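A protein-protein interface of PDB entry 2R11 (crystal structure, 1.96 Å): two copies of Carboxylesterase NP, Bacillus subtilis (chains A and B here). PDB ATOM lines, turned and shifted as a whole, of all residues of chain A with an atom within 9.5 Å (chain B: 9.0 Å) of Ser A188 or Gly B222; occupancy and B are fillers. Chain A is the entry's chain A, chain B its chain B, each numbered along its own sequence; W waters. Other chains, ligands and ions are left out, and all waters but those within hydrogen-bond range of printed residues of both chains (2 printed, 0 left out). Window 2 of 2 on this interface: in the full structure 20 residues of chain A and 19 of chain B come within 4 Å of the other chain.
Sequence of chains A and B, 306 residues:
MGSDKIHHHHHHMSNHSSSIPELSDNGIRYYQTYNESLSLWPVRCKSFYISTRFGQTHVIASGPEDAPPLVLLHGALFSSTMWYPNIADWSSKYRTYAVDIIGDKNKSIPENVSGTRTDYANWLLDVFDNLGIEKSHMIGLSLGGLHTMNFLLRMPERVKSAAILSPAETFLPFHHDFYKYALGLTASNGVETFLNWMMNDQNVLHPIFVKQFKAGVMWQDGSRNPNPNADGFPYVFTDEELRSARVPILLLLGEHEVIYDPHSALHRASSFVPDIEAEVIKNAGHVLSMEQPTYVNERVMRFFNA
The backbone carbonyl oxygen (O) of Gln B220 lies within hydrogen-bond range of the backbone NH (N) of Ser A188, 3.2 Å away.
OG of Ser A188 lies close to O of Asp B221.
The side-chain hydroxyl (OG) of Ser A188 is in hydrogen-bond range of the backbone carbonyl oxygen (O) of Gly B222, at 2.9 Å.
O of Asn A189 is in hydrogen-bond range of OG1 of Thr A193 (2.5 Å).
The side-chain carboxylate (OD1) of Asp B221 is in hydrogen-bond range of the side-chain hydroxyl (OG) of Ser B24 (2.6 Å).
The side-chain carboxylate (OD1) of Asp B221 sits close to the indole nitrogen (NE1) of Trp B219.
Of the 15 printed residues of chain A, 5 touch a printed residue of chain B.
Hydrophobic or aromatic side chains of chain A within 4 Å of the printed part of chain B: Ala A187.
Of the 26 printed residues of chain B, 6 touch a printed residue of chain A.
Among the printed residues, 9 pairs touch across the chains.
Among the printed residues, no Asp or Glu carboxylate lies within 4 Å of a Lys or Arg side-chain nitrogen of the other chain.
Position printed for both chains: 218.
Thr A186 touches Gln B220 (O to CB, 3.4 Å).
Ala A187 touches Gln B220 (CA to O, 3.4 Å).
Asn B225 touches Ala A187.
Arg B224 touches Ser A188.
Arg B224 touches Asn A189.
Asn B227 touches Thr A193 (OD1 to CG2, 3.6 Å).
Ser A188 touches just these residues of chain B: Gln B220 (3.2 Å), Asp B221 (3.2 Å), Gly B222 (2.9 Å) and Arg B224 (3.5 Å).
Gly B222 touches just one residue of chain A: Ser A188 (2.9 Å).
Asp B221 touches one residue of chain A.
Of the printed residues of chain A, Arg B224 touches Ser A188 (3.5 Å) and Asn A189 (3.7 Å).
Of the printed residues of chain B, Asn A189 touches Arg B224 (3.7 Å).
Of the printed residues of chain A, Gln B220 touches Thr A186 (3.4 Å), Ala A187 (3.4 Å) and Ser A188 (3.2 Å).
Of the printed residues of chain A, Asn B227 touches Thr A193.
Gly B27 touches none of the printed residues of chain A.
Gly B216 touches none of the printed residues of chain A.
The nearest residue of chain B that does not touch Ser A188 is Ser B223 (4.3 Å).
Water W1 bridges the backbone carbonyl oxygen of Gly A184 and the side-chain amide nitrogen of Asn B225.
Water W2 bridges the backbone carbonyl oxygen (O) of Ser A188 (2.7 Å) and the backbone NH (N) of Asn B225 (3.4 Å).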
ATOM      1  N   LEU A 183     -14.386  16.184   6.759  1.00  0.00           N
ATOM      2  CA  LEU A 183     -14.025  16.778   5.477  1.00  0.00           C
ATOM      3  C   LEU A 183     -12.899  16.029   4.782  1.00  0.00           C
ATOM      4  O   LEU A 183     -12.801  16.058   3.558  1.00  0.00           O
ATOM      5  CB  LEU A 183     -13.663  18.266   5.641  1.00  0.00           C
ATOM      6  CG  LEU A 183     -14.838  19.250   5.572  1.00  0.00           C
ATOM      7  CD1 LEU A 183     -14.415  20.632   6.035  1.00  0.00           C
ATOM      8  CD2 LEU A 183     -15.409  19.320   4.148  1.00  0.00           C
ATOM      9  N   GLY A 184     -12.050  15.373   5.567  1.00  0.00           N
ATOM     10  CA  GLY A 184     -10.973  14.572   5.042  1.00  0.00           C
ATOM     11  C   GLY A 184     -11.379  13.136   4.723  1.00  0.00           C
ATOM     12  O   GLY A 184     -10.541  12.371   4.278  1.00  0.00           O
ATOM     13  N   LEU A 185     -12.644  12.758   4.945  1.00  0.00           N
ATOM     14  CA  LEU A 185     -13.105  11.399   4.614  1.00  0.00           C
ATOM     15  C   LEU A 185     -12.826  10.973   3.176  1.00  0.00           C
ATOM     16  O   LEU A 185     -12.430   9.828   2.939  1.00  0.00           O
ATOM     17  CB  LEU A 185     -14.617  11.244   4.830  1.00  0.00           C
ATOM     18  CG  LEU A 185     -15.082  10.772   6.212  1.00  0.00           C
ATOM     19  CD1 LEU A 185     -16.611  10.748   6.269  1.00  0.00           C
ATOM     20  CD2 LEU A 185     -14.529   9.394   6.521  1.00  0.00           C
ATOM     21  N   THR A 186     -13.098  11.886   2.244  1.00  0.00           N
ATOM     22  CA  THR A 186     -12.948  11.687   0.797  1.00  0.00           C
ATOM     23  C   THR A 186     -11.562  12.102   0.317  1.00  0.00           C
ATOM     24  O   THR A 186     -11.429  12.979  -0.555  1.00  0.00           O
ATOM     25  CB  THR A 186     -13.947  12.557   0.037  1.00  0.00           C
ATOM     26  OG1 THR A 186     -13.743  13.924   0.428  1.00  0.00           O
ATOM     27  CG2 THR A 186     -15.387  12.145   0.353  1.00  0.00           C
ATOM     28  N   ALA A 187     -10.533  11.511   0.919  1.00  0.00           N
ATOM     29  CA  ALA A 187      -9.143  11.732   0.518  1.00  0.00           C
ATOM     30  C   ALA A 187      -8.423  10.427   0.778  1.00  0.00           C
ATOM     31  O   ALA A 187      -8.938   9.589   1.521  1.00  0.00           O
ATOM     32  CB  ALA A 187      -8.508  12.852   1.311  1.00  0.00           C
ATOM     33  N   SER A 188      -7.254  10.238   0.164  1.00  0.00           N
ATOM     34  CA  SER A 188      -6.450   9.034   0.411  1.00  0.00           C
ATOM     35  C   SER A 188      -6.189   8.945   1.901  1.00  0.00           C
ATOM     36  O   SER A 188      -5.678   9.906   2.500  1.00  0.00           O
ATOM     37  CB  SER A 188      -5.102   9.079  -0.326  1.00  0.00           C
ATOM     38  OG  SER A 188      -5.274   9.471  -1.679  1.00  0.00           O
ATOM     39  N   ASN A 189      -6.555   7.805   2.483  1.00  0.00           N
ATOM     40  CA  ASN A 189      -6.345   7.517   3.900  1.00  0.00           C
ATOM     41  C   ASN A 189      -7.303   8.300   4.806  1.00  0.00           C
ATOM     42  O   ASN A 189      -7.093   8.408   6.003  1.00  0.00           O
ATOM     43  CB  ASN A 189      -4.880   7.798   4.274  1.00  0.00           C
ATOM     44  CG  ASN A 189      -4.473   7.162   5.581  1.00  0.00           C
ATOM     45  OD1 ASN A 189      -4.663   5.961   5.783  1.00  0.00           O
ATOM     46  ND2 ASN A 189      -3.887   7.964   6.475  1.00  0.00           N
ATOM     47  N   GLY A 190      -8.373   8.823   4.228  1.00  0.00           N
ATOM     48  CA  GLY A 190      -9.352   9.613   4.980  1.00  0.00           C
ATOM     49  C   GLY A 190     -10.286   8.802   5.861  1.00  0.00           C
ATOM     50  O   GLY A 190     -10.619   9.229   6.970  1.00  0.00           O
ATOM     51  N   VAL A 191     -10.736   7.645   5.374  1.00  0.00           N
ATOM     52  CA  VAL A 191     -11.599   6.790   6.176  1.00  0.00           C
ATOM     53  C   VAL A 191     -10.798   6.216   7.354  1.00  0.00           C
ATOM     54  O   VAL A 191     -11.262   6.211   8.500  1.00  0.00           O
ATOM     55  CB  VAL A 191     -12.281   5.695   5.309  1.00  0.00           C
ATOM     56  CG1 VAL A 191     -12.843   4.594   6.154  1.00  0.00           C
ATOM     57  CG2 VAL A 191     -13.357   6.322   4.455  1.00  0.00           C
ATOM     58  N   GLU A 192      -9.583   5.748   7.085  1.00  0.00           N
ATOM     59  CA  GLU A 192      -8.724   5.198   8.137  1.00  0.00           C
ATOM     60  C   GLU A 192      -8.474   6.272   9.200  1.00  0.00           C
ATOM     61  O   GLU A 192      -8.657   6.042  10.385  1.00  0.00           O
ATOM     62  CB  GLU A 192      -7.392   4.705   7.535  1.00  0.00           C
ATOM     63  N   THR A 193      -8.083   7.462   8.755  1.00  0.00           N
ATOM     64  CA  THR A 193      -7.882   8.598   9.641  1.00  0.00           C
ATOM     65  C   THR A 193      -9.141   8.929  10.470  1.00  0.00           C
ATOM     66  O   THR A 193      -9.063   9.077  11.687  1.00  0.00           O
ATOM     67  CB  THR A 193      -7.438   9.843   8.808  1.00  0.00           C
ATOM     68  OG1 THR A 193      -6.234   9.520   8.105  1.00  0.00           O
ATOM     69  CG2 THR A 193      -7.210  11.081   9.683  1.00  0.00           C
ATOM     70  N   PHE A 194     -10.291   9.012   9.802  1.00  0.00           N
ATOM     71  CA  PHE A 194     -11.552   9.350  10.446  1.00  0.00           C
ATOM     72  C   PHE A 194     -11.895   8.336  11.524  1.00  0.00           C
ATOM     73  O   PHE A 194     -12.169   8.711  12.668  1.00  0.00           O
ATOM     74  CB  PHE A 194     -12.681   9.392   9.390  1.00  0.00           C
ATOM     75  CG  PHE A 194     -14.048   9.728   9.955  1.00  0.00           C
ATOM     76  CD1 PHE A 194     -14.441  11.053  10.143  1.00  0.00           C
ATOM     77  CD2 PHE A 194     -14.939   8.723  10.269  1.00  0.00           C
ATOM     78  CE1 PHE A 194     -15.703  11.359  10.653  1.00  0.00           C
ATOM     79  CE2 PHE A 194     -16.215   9.022  10.779  1.00  0.00           C
ATOM     80  CZ  PHE A 194     -16.594  10.338  10.967  1.00  0.00           C
ATOM     81  N   LYS A 214     -16.371   2.426   3.635  1.00  0.00           N
ATOM     82  CA  LYS A 214     -15.550   3.039   2.587  1.00  0.00           C
ATOM     83  C   LYS A 214     -16.260   3.144   1.234  1.00  0.00           C
ATOM     84  O   LYS A 214     -16.137   4.173   0.550  1.00  0.00           O
ATOM     85  CB  LYS A 214     -14.244   2.245   2.427  1.00  0.00           C
ATOM     86  CG  LYS A 214     -13.326   2.741   1.299  1.00  0.00           C
ATOM     87  CD  LYS A 214     -12.993   4.229   1.416  1.00  0.00           C
ATOM     88  CE  LYS A 214     -11.841   4.611   0.492  1.00  0.00           C
ATOM     89  NZ  LYS A 214     -10.543   4.057   0.953  1.00  0.00           N
ATOM     90  N   VAL A 217     -18.596   5.948   1.280  1.00  0.00           N
ATOM     91  CA  VAL A 217     -17.877   7.209   1.144  1.00  0.00           C
ATOM     92  C   VAL A 217     -17.507   7.439  -0.320  1.00  0.00           C
ATOM     93  O   VAL A 217     -17.625   8.547  -0.807  1.00  0.00           O
ATOM     94  CB  VAL A 217     -16.629   7.273   2.069  1.00  0.00           C
ATOM     95  CG1 VAL A 217     -15.808   8.522   1.777  1.00  0.00           C
ATOM     96  CG2 VAL A 217     -17.044   7.234   3.565  1.00  0.00           C
ATOM     97  N   MET A 218     -17.104   6.385  -1.021  1.00  0.00           N
ATOM     98  CA  MET A 218     -16.767   6.453  -2.455  1.00  0.00           C
ATOM     99  C   MET A 218     -17.995   6.762  -3.330  1.00  0.00           C
ATOM    100  O   MET A 218     -17.867   7.312  -4.445  1.00  0.00           O
ATOM    101  CB  MET A 218     -16.191   5.104  -2.919  1.00  0.00           C
ATOM    102  CG  MET A 218     -14.832   4.729  -2.346  1.00  0.00           C
ATOM    103  SD  MET A 218     -13.451   5.867  -3.094  1.00  0.00           S
ATOM    104  CE  MET A 218     -13.854   5.585  -5.025  1.00  0.00           C
ATOM    105  N   ILE B  20       3.174   9.262  -2.249  1.00  0.00           N
ATOM    106  CA  ILE B  20       3.364   9.931  -3.579  1.00  0.00           C
ATOM    107  C   ILE B  20       2.937   9.015  -4.735  1.00  0.00           C
ATOM    108  O   ILE B  20       3.781   8.433  -5.414  1.00  0.00           O
ATOM    109  CB  ILE B  20       4.833  10.351  -3.780  1.00  0.00           C
ATOM    110  N   PRO B  21       1.614   8.888  -4.964  1.00  0.00           N
ATOM    111  CA  PRO B  21       1.112   7.975  -6.007  1.00  0.00           C
ATOM    112  C   PRO B  21       1.191   8.538  -7.424  1.00  0.00           C
ATOM    113  O   PRO B  21       1.120   9.758  -7.598  1.00  0.00           O
ATOM    114  CB  PRO B  21      -0.355   7.758  -5.604  1.00  0.00           C
ATOM    115  CG  PRO B  21      -0.742   9.006  -4.833  1.00  0.00           C
ATOM    116  CD  PRO B  21       0.521   9.603  -4.263  1.00  0.00           C
ATOM    117  N   GLU B  22       1.356   7.651  -8.415  1.00  0.00           N
ATOM    118  CA  GLU B  22       1.279   8.018  -9.835  1.00  0.00           C
ATOM    119  C   GLU B  22      -0.016   8.800 -10.009  1.00  0.00           C
ATOM    120  O   GLU B  22      -0.986   8.556  -9.279  1.00  0.00           O
ATOM    121  CB  GLU B  22       1.223   6.762 -10.714  1.00  0.00           C
ATOM    122  N   LEU B  23      -0.056   9.728 -10.965  1.00  0.00           N
ATOM    123  CA  LEU B  23      -1.255  10.548 -11.135  1.00  0.00           C
ATOM    124  C   LEU B  23      -2.440   9.732 -11.685  1.00  0.00           C
ATOM    125  O   LEU B  23      -2.377   9.170 -12.779  1.00  0.00           O
ATOM    126  CB  LEU B  23      -0.958  11.748 -12.033  1.00  0.00           C
ATOM    127  CG  LEU B  23      -1.908  12.936 -12.015  1.00  0.00           C
ATOM    128  CD1 LEU B  23      -2.055  13.520 -10.577  1.00  0.00           C
ATOM    129  CD2 LEU B  23      -1.407  13.995 -13.013  1.00  0.00           C
ATOM    130  N   SER B  24      -3.520   9.676 -10.914  1.00  0.00           N
ATOM    131  CA  SER B  24      -4.732   8.965 -11.325  1.00  0.00           C
ATOM    132  C   SER B  24      -5.385   9.628 -12.515  1.00  0.00           C
ATOM    133  O   SER B  24      -4.973  10.697 -12.938  1.00  0.00           O
ATOM    134  CB  SER B  24      -5.746   8.952 -10.189  1.00  0.00           C
ATOM    135  OG  SER B  24      -6.304  10.236  -9.996  1.00  0.00           O
ATOM    136  N   ASN B  26      -8.348  10.936 -12.411  1.00  0.00           N
ATOM    137  CA  ASN B  26      -8.961  12.181 -11.930  1.00  0.00           C
ATOM    138  C   ASN B  26      -7.896  13.283 -11.767  1.00  0.00           C
ATOM    139  O   ASN B  26      -8.172  14.461 -12.021  1.00  0.00           O
ATOM    140  CB  ASN B  26      -9.773  11.953 -10.642  1.00  0.00           C
ATOM    141  CG  ASN B  26     -11.102  11.221 -10.903  1.00  0.00           C
ATOM    142  OD1 ASN B  26     -11.605  11.209 -12.015  1.00  0.00           O
ATOM    143  ND2 ASN B  26     -11.656  10.599  -9.875  1.00  0.00           N
ATOM    144  N   GLY B  27      -6.694  12.879 -11.350  1.00  0.00           N
ATOM    145  CA  GLY B  27      -5.533  13.766 -11.230  1.00  0.00           C
ATOM    146  C   GLY B  27      -5.147  14.314 -12.585  1.00  0.00           C
ATOM    147  O   GLY B  27      -4.884  15.498 -12.730  1.00  0.00           O
ATOM    148  N   TYR B  31      -5.279  18.263 -13.764  1.00  0.00           N
ATOM    149  CA  TYR B  31      -4.128  18.925 -14.372  1.00  0.00           C
ATOM    150  C   TYR B  31      -4.558  19.563 -15.707  1.00  0.00           C
ATOM    151  O   TYR B  31      -4.153  20.675 -16.027  1.00  0.00           O
ATOM    152  CB  TYR B  31      -2.944  17.948 -14.504  1.00  0.00           C
ATOM    153  CG  TYR B  31      -2.014  17.930 -13.302  1.00  0.00           C
ATOM    154  CD1 TYR B  31      -2.504  17.768 -12.003  1.00  0.00           C
ATOM    155  CD2 TYR B  31      -0.632  18.065 -13.466  1.00  0.00           C
ATOM    156  CE1 TYR B  31      -1.646  17.747 -10.888  1.00  0.00           C
ATOM    157  CE2 TYR B  31       0.233  18.047 -12.370  1.00  0.00           C
ATOM    158  CZ  TYR B  31      -0.278  17.896 -11.091  1.00  0.00           C
ATOM    159  OH  TYR B  31       0.579  17.891 -10.029  1.00  0.00           O
ATOM    160  N   GLY B 103       0.235  21.066  -0.057  1.00  0.00           N
ATOM    161  CA  GLY B 103      -0.793  20.219   0.556  1.00  0.00           C
ATOM    162  C   GLY B 103      -2.235  20.544   0.164  1.00  0.00           C
ATOM    163  O   GLY B 103      -3.137  19.723   0.355  1.00  0.00           O
ATOM    164  N   ASP B 104      -2.478  21.740  -0.361  1.00  0.00           N
ATOM    165  CA  ASP B 104      -3.845  22.089  -0.813  1.00  0.00           C
ATOM    166  C   ASP B 104      -4.113  21.503  -2.231  1.00  0.00           C
ATOM    167  O   ASP B 104      -3.197  20.970  -2.877  1.00  0.00           O
ATOM    168  CB  ASP B 104      -4.019  23.615  -0.731  1.00  0.00           C
ATOM    169  CG  ASP B 104      -5.463  24.078  -0.893  1.00  0.00           C
ATOM    170  OD1 ASP B 104      -6.417  23.320  -0.620  1.00  0.00           O
ATOM    171  OD2 ASP B 104      -5.649  25.235  -1.295  1.00  0.00           O
ATOM    172  N   LYS B 105      -5.354  21.566  -2.711  1.00  0.00           N
ATOM    173  CA  LYS B 105      -5.690  20.997  -4.026  1.00  0.00           C
ATOM    174  C   LYS B 105      -5.163  21.881  -5.153  1.00  0.00           C
ATOM    175  O   LYS B 105      -5.787  22.885  -5.532  1.00  0.00           O
ATOM    176  CB  LYS B 105      -7.199  20.799  -4.161  1.00  0.00           C
ATOM    177  CG  LYS B 105      -7.639  19.859  -5.297  1.00  0.00           C
ATOM    178  CD  LYS B 105      -7.115  18.436  -5.139  1.00  0.00           C
ATOM    179  CE  LYS B 105      -7.603  17.737  -3.883  1.00  0.00           C
ATOM    180  NZ  LYS B 105      -9.089  17.535  -3.821  1.00  0.00           N
ATOM    181  N   ASN B 106      -4.004  21.516  -5.683  1.00  0.00           N
ATOM    182  CA  ASN B 106      -3.332  22.330  -6.700  1.00  0.00           C
ATOM    183  C   ASN B 106      -2.150  21.541  -7.272  1.00  0.00           C
ATOM    184  O   ASN B 106      -2.098  20.317  -7.106  1.00  0.00           O
ATOM    185  CB  ASN B 106      -2.913  23.687  -6.095  1.00  0.00           C
ATOM    186  CG  ASN B 106      -1.982  23.540  -4.897  1.00  0.00           C
ATOM    187  OD1 ASN B 106      -1.074  22.729  -4.925  1.00  0.00           O
ATOM    188  ND2 ASN B 106      -2.172  24.370  -3.867  1.00  0.00           N
ATOM    189  N   SER B 108       1.104  21.759  -6.433  1.00  0.00           N
ATOM    190  CA  SER B 108       2.228  21.477  -5.514  1.00  0.00           C
ATOM    191  C   SER B 108       2.164  20.030  -4.985  1.00  0.00           C
ATOM    192  O   SER B 108       1.090  19.482  -4.755  1.00  0.00           O
ATOM    193  CB  SER B 108       2.285  22.478  -4.365  1.00  0.00           C
ATOM    194  OG  SER B 108       2.718  23.749  -4.815  1.00  0.00           O
ATOM    195  N   ILE B 109       3.334  19.425  -4.783  1.00  0.00           N
ATOM    196  CA  ILE B 109       3.418  18.024  -4.385  1.00  0.00           C
ATOM    197  C   ILE B 109       3.994  17.935  -2.978  1.00  0.00           C
ATOM    198  O   ILE B 109       5.195  18.107  -2.781  1.00  0.00           O
ATOM    199  CB  ILE B 109       4.288  17.240  -5.375  1.00  0.00           C
ATOM    200  CG1 ILE B 109       3.710  17.366  -6.783  1.00  0.00           C
ATOM    201  CG2 ILE B 109       4.348  15.772  -5.003  1.00  0.00           C
ATOM    202  CD1 ILE B 109       4.637  16.871  -7.837  1.00  0.00           C
ATOM    203  N   PRO B 110       3.138  17.665  -1.991  1.00  0.00           N
ATOM    204  CA  PRO B 110       3.606  17.656  -0.622  1.00  0.00           C
ATOM    205  C   PRO B 110       4.351  16.375  -0.280  1.00  0.00           C
ATOM    206  O   PRO B 110       4.062  15.323  -0.858  1.00  0.00           O
ATOM    207  CB  PRO B 110       2.314  17.767   0.183  1.00  0.00           C
ATOM    208  CG  PRO B 110       1.280  17.096  -0.658  1.00  0.00           C
ATOM    209  CD  PRO B 110       1.699  17.349  -2.090  1.00  0.00           C
ATOM    210  N   GLY B 216     -10.912  19.482  -9.113  1.00  0.00           N
ATOM    211  CA  GLY B 216     -10.126  19.307  -7.901  1.00  0.00           C
ATOM    212  C   GLY B 216     -10.936  18.588  -6.832  1.00  0.00           C
ATOM    213  O   GLY B 216     -10.419  17.701  -6.172  1.00  0.00           O
ATOM    214  N   MET B 218     -13.253  16.469  -7.255  1.00  0.00           N
ATOM    215  CA  MET B 218     -13.367  15.075  -7.670  1.00  0.00           C
ATOM    216  C   MET B 218     -12.035  14.332  -7.652  1.00  0.00           C
ATOM    217  O   MET B 218     -12.019  13.119  -7.796  1.00  0.00           O
ATOM    218  CB  MET B 218     -13.984  14.985  -9.056  1.00  0.00           C
ATOM    219  CG  MET B 218     -15.357  15.604  -9.135  1.00  0.00           C
ATOM    220  SD  MET B 218     -16.221  15.138 -10.790  1.00  0.00           S
ATOM    221  CE  MET B 218     -16.551  13.261 -10.409  1.00  0.00           C
ATOM    222  N   TRP B 219     -10.923  15.052  -7.479  1.00  0.00           N
ATOM    223  CA  TRP B 219      -9.610  14.417  -7.408  1.00  0.00           C
ATOM    224  C   TRP B 219      -9.307  14.095  -5.949  1.00  0.00           C
ATOM    225  O   TRP B 219      -8.707  14.890  -5.210  1.00  0.00           O
ATOM    226  CB  TRP B 219      -8.525  15.263  -8.088  1.00  0.00           C
ATOM    227  CG  TRP B 219      -7.132  14.658  -7.994  1.00  0.00           C
ATOM    228  CD1 TRP B 219      -6.812  13.339  -7.980  1.00  0.00           C
ATOM    229  CD2 TRP B 219      -5.884  15.376  -7.951  1.00  0.00           C
ATOM    230  NE1 TRP B 219      -5.438  13.176  -7.896  1.00  0.00           N
ATOM    231  CE2 TRP B 219      -4.849  14.416  -7.893  1.00  0.00           C
ATOM    232  CE3 TRP B 219      -5.552  16.730  -7.944  1.00  0.00           C
ATOM    233  CZ2 TRP B 219      -3.513  14.769  -7.801  1.00  0.00           C
ATOM    234  CZ3 TRP B 219      -4.205  17.085  -7.874  1.00  0.00           C
ATOM    235  CH2 TRP B 219      -3.206  16.105  -7.808  1.00  0.00           C
ATOM    236  N   GLN B 220      -9.728  12.897  -5.549  1.00  0.00           N
ATOM    237  CA  GLN B 220      -9.650  12.466  -4.166  1.00  0.00           C
ATOM    238  C   GLN B 220      -8.586  11.402  -3.857  1.00  0.00           C
ATOM    239  O   GLN B 220      -8.462  10.985  -2.712  1.00  0.00           O
ATOM    240  CB  GLN B 220     -11.037  11.970  -3.750  1.00  0.00           C
ATOM    241  CG  GLN B 220     -12.110  13.061  -3.913  1.00  0.00           C
ATOM    242  CD  GLN B 220     -13.529  12.530  -3.832  1.00  0.00           C
ATOM    243  OE1 GLN B 220     -13.768  11.411  -3.385  1.00  0.00           O
ATOM    244  NE2 GLN B 220     -14.488  13.356  -4.248  1.00  0.00           N
ATOM    245  N   ASP B 221      -7.811  10.980  -4.850  1.00  0.00           N
ATOM    246  CA  ASP B 221      -6.820   9.904  -4.645  1.00  0.00           C
ATOM    247  C   ASP B 221      -5.367  10.376  -4.754  1.00  0.00           C
ATOM    248  O   ASP B 221      -4.483   9.587  -5.042  1.00  0.00           O
ATOM    249  CB  ASP B 221      -7.085   8.736  -5.613  1.00  0.00           C
ATOM    250  CG  ASP B 221      -7.258   9.188  -7.057  1.00  0.00           C
ATOM    251  OD1 ASP B 221      -6.775  10.290  -7.415  1.00  0.00           O
ATOM    252  OD2 ASP B 221      -7.900   8.451  -7.839  1.00  0.00           O
ATOM    253  N   GLY B 222      -5.118  11.655  -4.519  1.00  0.00           N
ATOM    254  CA  GLY B 222      -3.760  12.191  -4.585  1.00  0.00           C
ATOM    255  C   GLY B 222      -3.080  12.089  -3.237  1.00  0.00           C
ATOM    256  O   GLY B 222      -3.054  11.027  -2.625  1.00  0.00           O
ATOM    257  N   SER B 223      -2.542  13.210  -2.766  1.00  0.00           N
ATOM    258  CA  SER B 223      -1.871  13.263  -1.469  1.00  0.00           C
ATOM    259  C   SER B 223      -2.827  13.075  -0.291  1.00  0.00           C
ATOM    260  O   SER B 223      -4.027  13.344  -0.388  1.00  0.00           O
ATOM    261  CB  SER B 223      -1.176  14.619  -1.292  1.00  0.00           C
ATOM    262  OG  SER B 223      -0.433  14.989  -2.440  1.00  0.00           O
ATOM    263  N   ARG B 224      -2.277  12.594   0.818  1.00  0.00           N
ATOM    264  CA  ARG B 224      -2.995  12.571   2.078  1.00  0.00           C
ATOM    265  C   ARG B 224      -2.990  13.992   2.622  1.00  0.00           C
ATOM    266  O   ARG B 224      -2.139  14.798   2.255  1.00  0.00           O
ATOM    267  CB  ARG B 224      -2.293  11.688   3.105  1.00  0.00           C
ATOM    268  CG  ARG B 224      -2.187  10.226   2.762  1.00  0.00           C
ATOM    269  CD  ARG B 224      -1.568   9.488   3.939  1.00  0.00           C
ATOM    270  NE  ARG B 224      -1.245   8.102   3.627  1.00  0.00           N
ATOM    271  CZ  ARG B 224      -0.606   7.277   4.456  1.00  0.00           C
ATOM    272  NH1 ARG B 224      -0.209   7.691   5.661  1.00  0.00           N
ATOM    273  NH2 ARG B 224      -0.356   6.029   4.080  1.00  0.00           N
ATOM    274  N   ASN B 225      -3.937  14.280   3.511  1.00  0.00           N
ATOM    275  CA  ASN B 225      -3.987  15.558   4.221  1.00  0.00           C
ATOM    276  C   ASN B 225      -3.246  15.399   5.541  1.00  0.00           C
ATOM    277  O   ASN B 225      -3.268  14.316   6.117  1.00  0.00           O
ATOM    278  CB  ASN B 225      -5.441  15.930   4.526  1.00  0.00           C
ATOM    279  CG  ASN B 225      -6.296  16.018   3.278  1.00  0.00           C
ATOM    280  OD1 ASN B 225      -5.940  16.693   2.318  1.00  0.00           O
ATOM    281  ND2 ASN B 225      -7.429  15.324   3.287  1.00  0.00           N
ATOM    282  N   PRO B 226      -2.561  16.457   6.019  1.00  0.00           N
ATOM    283  CA  PRO B 226      -2.070  16.309   7.388  1.00  0.00           C
ATOM    284  C   PRO B 226      -3.256  16.085   8.322  1.00  0.00           C
ATOM    285  O   PRO B 226      -4.348  16.592   8.057  1.00  0.00           O
ATOM    286  CB  PRO B 226      -1.398  17.655   7.694  1.00  0.00           C
ATOM    287  CG  PRO B 226      -1.742  18.573   6.564  1.00  0.00           C
ATOM    288  CD  PRO B 226      -2.179  17.740   5.406  1.00  0.00           C
ATOM    289  N   ASN B 227      -3.062  15.327   9.390  1.00  0.00           N
ATOM    290  CA  ASN B 227      -4.146  15.113  10.337  1.00  0.00           C
ATOM    291  C   ASN B 227      -4.542  16.434  10.971  1.00  0.00           C
ATOM    292  O   ASN B 227      -3.687  17.299  11.190  1.00  0.00           O
ATOM    293  CB  ASN B 227      -3.742  14.145  11.452  1.00  0.00           C
ATOM    294  CG  ASN B 227      -3.502  12.744  10.954  1.00  0.00           C
ATOM    295  OD1 ASN B 227      -3.822  12.401   9.813  1.00  0.00           O
ATOM    296  ND2 ASN B 227      -2.938  11.919  11.815  1.00  0.00           N
HETATM  297  O   HOH W   1      -8.076  13.066   4.923  1.00  0.00           O
HETATM  298  O   HOH W   2      -5.894  11.737   4.525  1.00  0.00           O
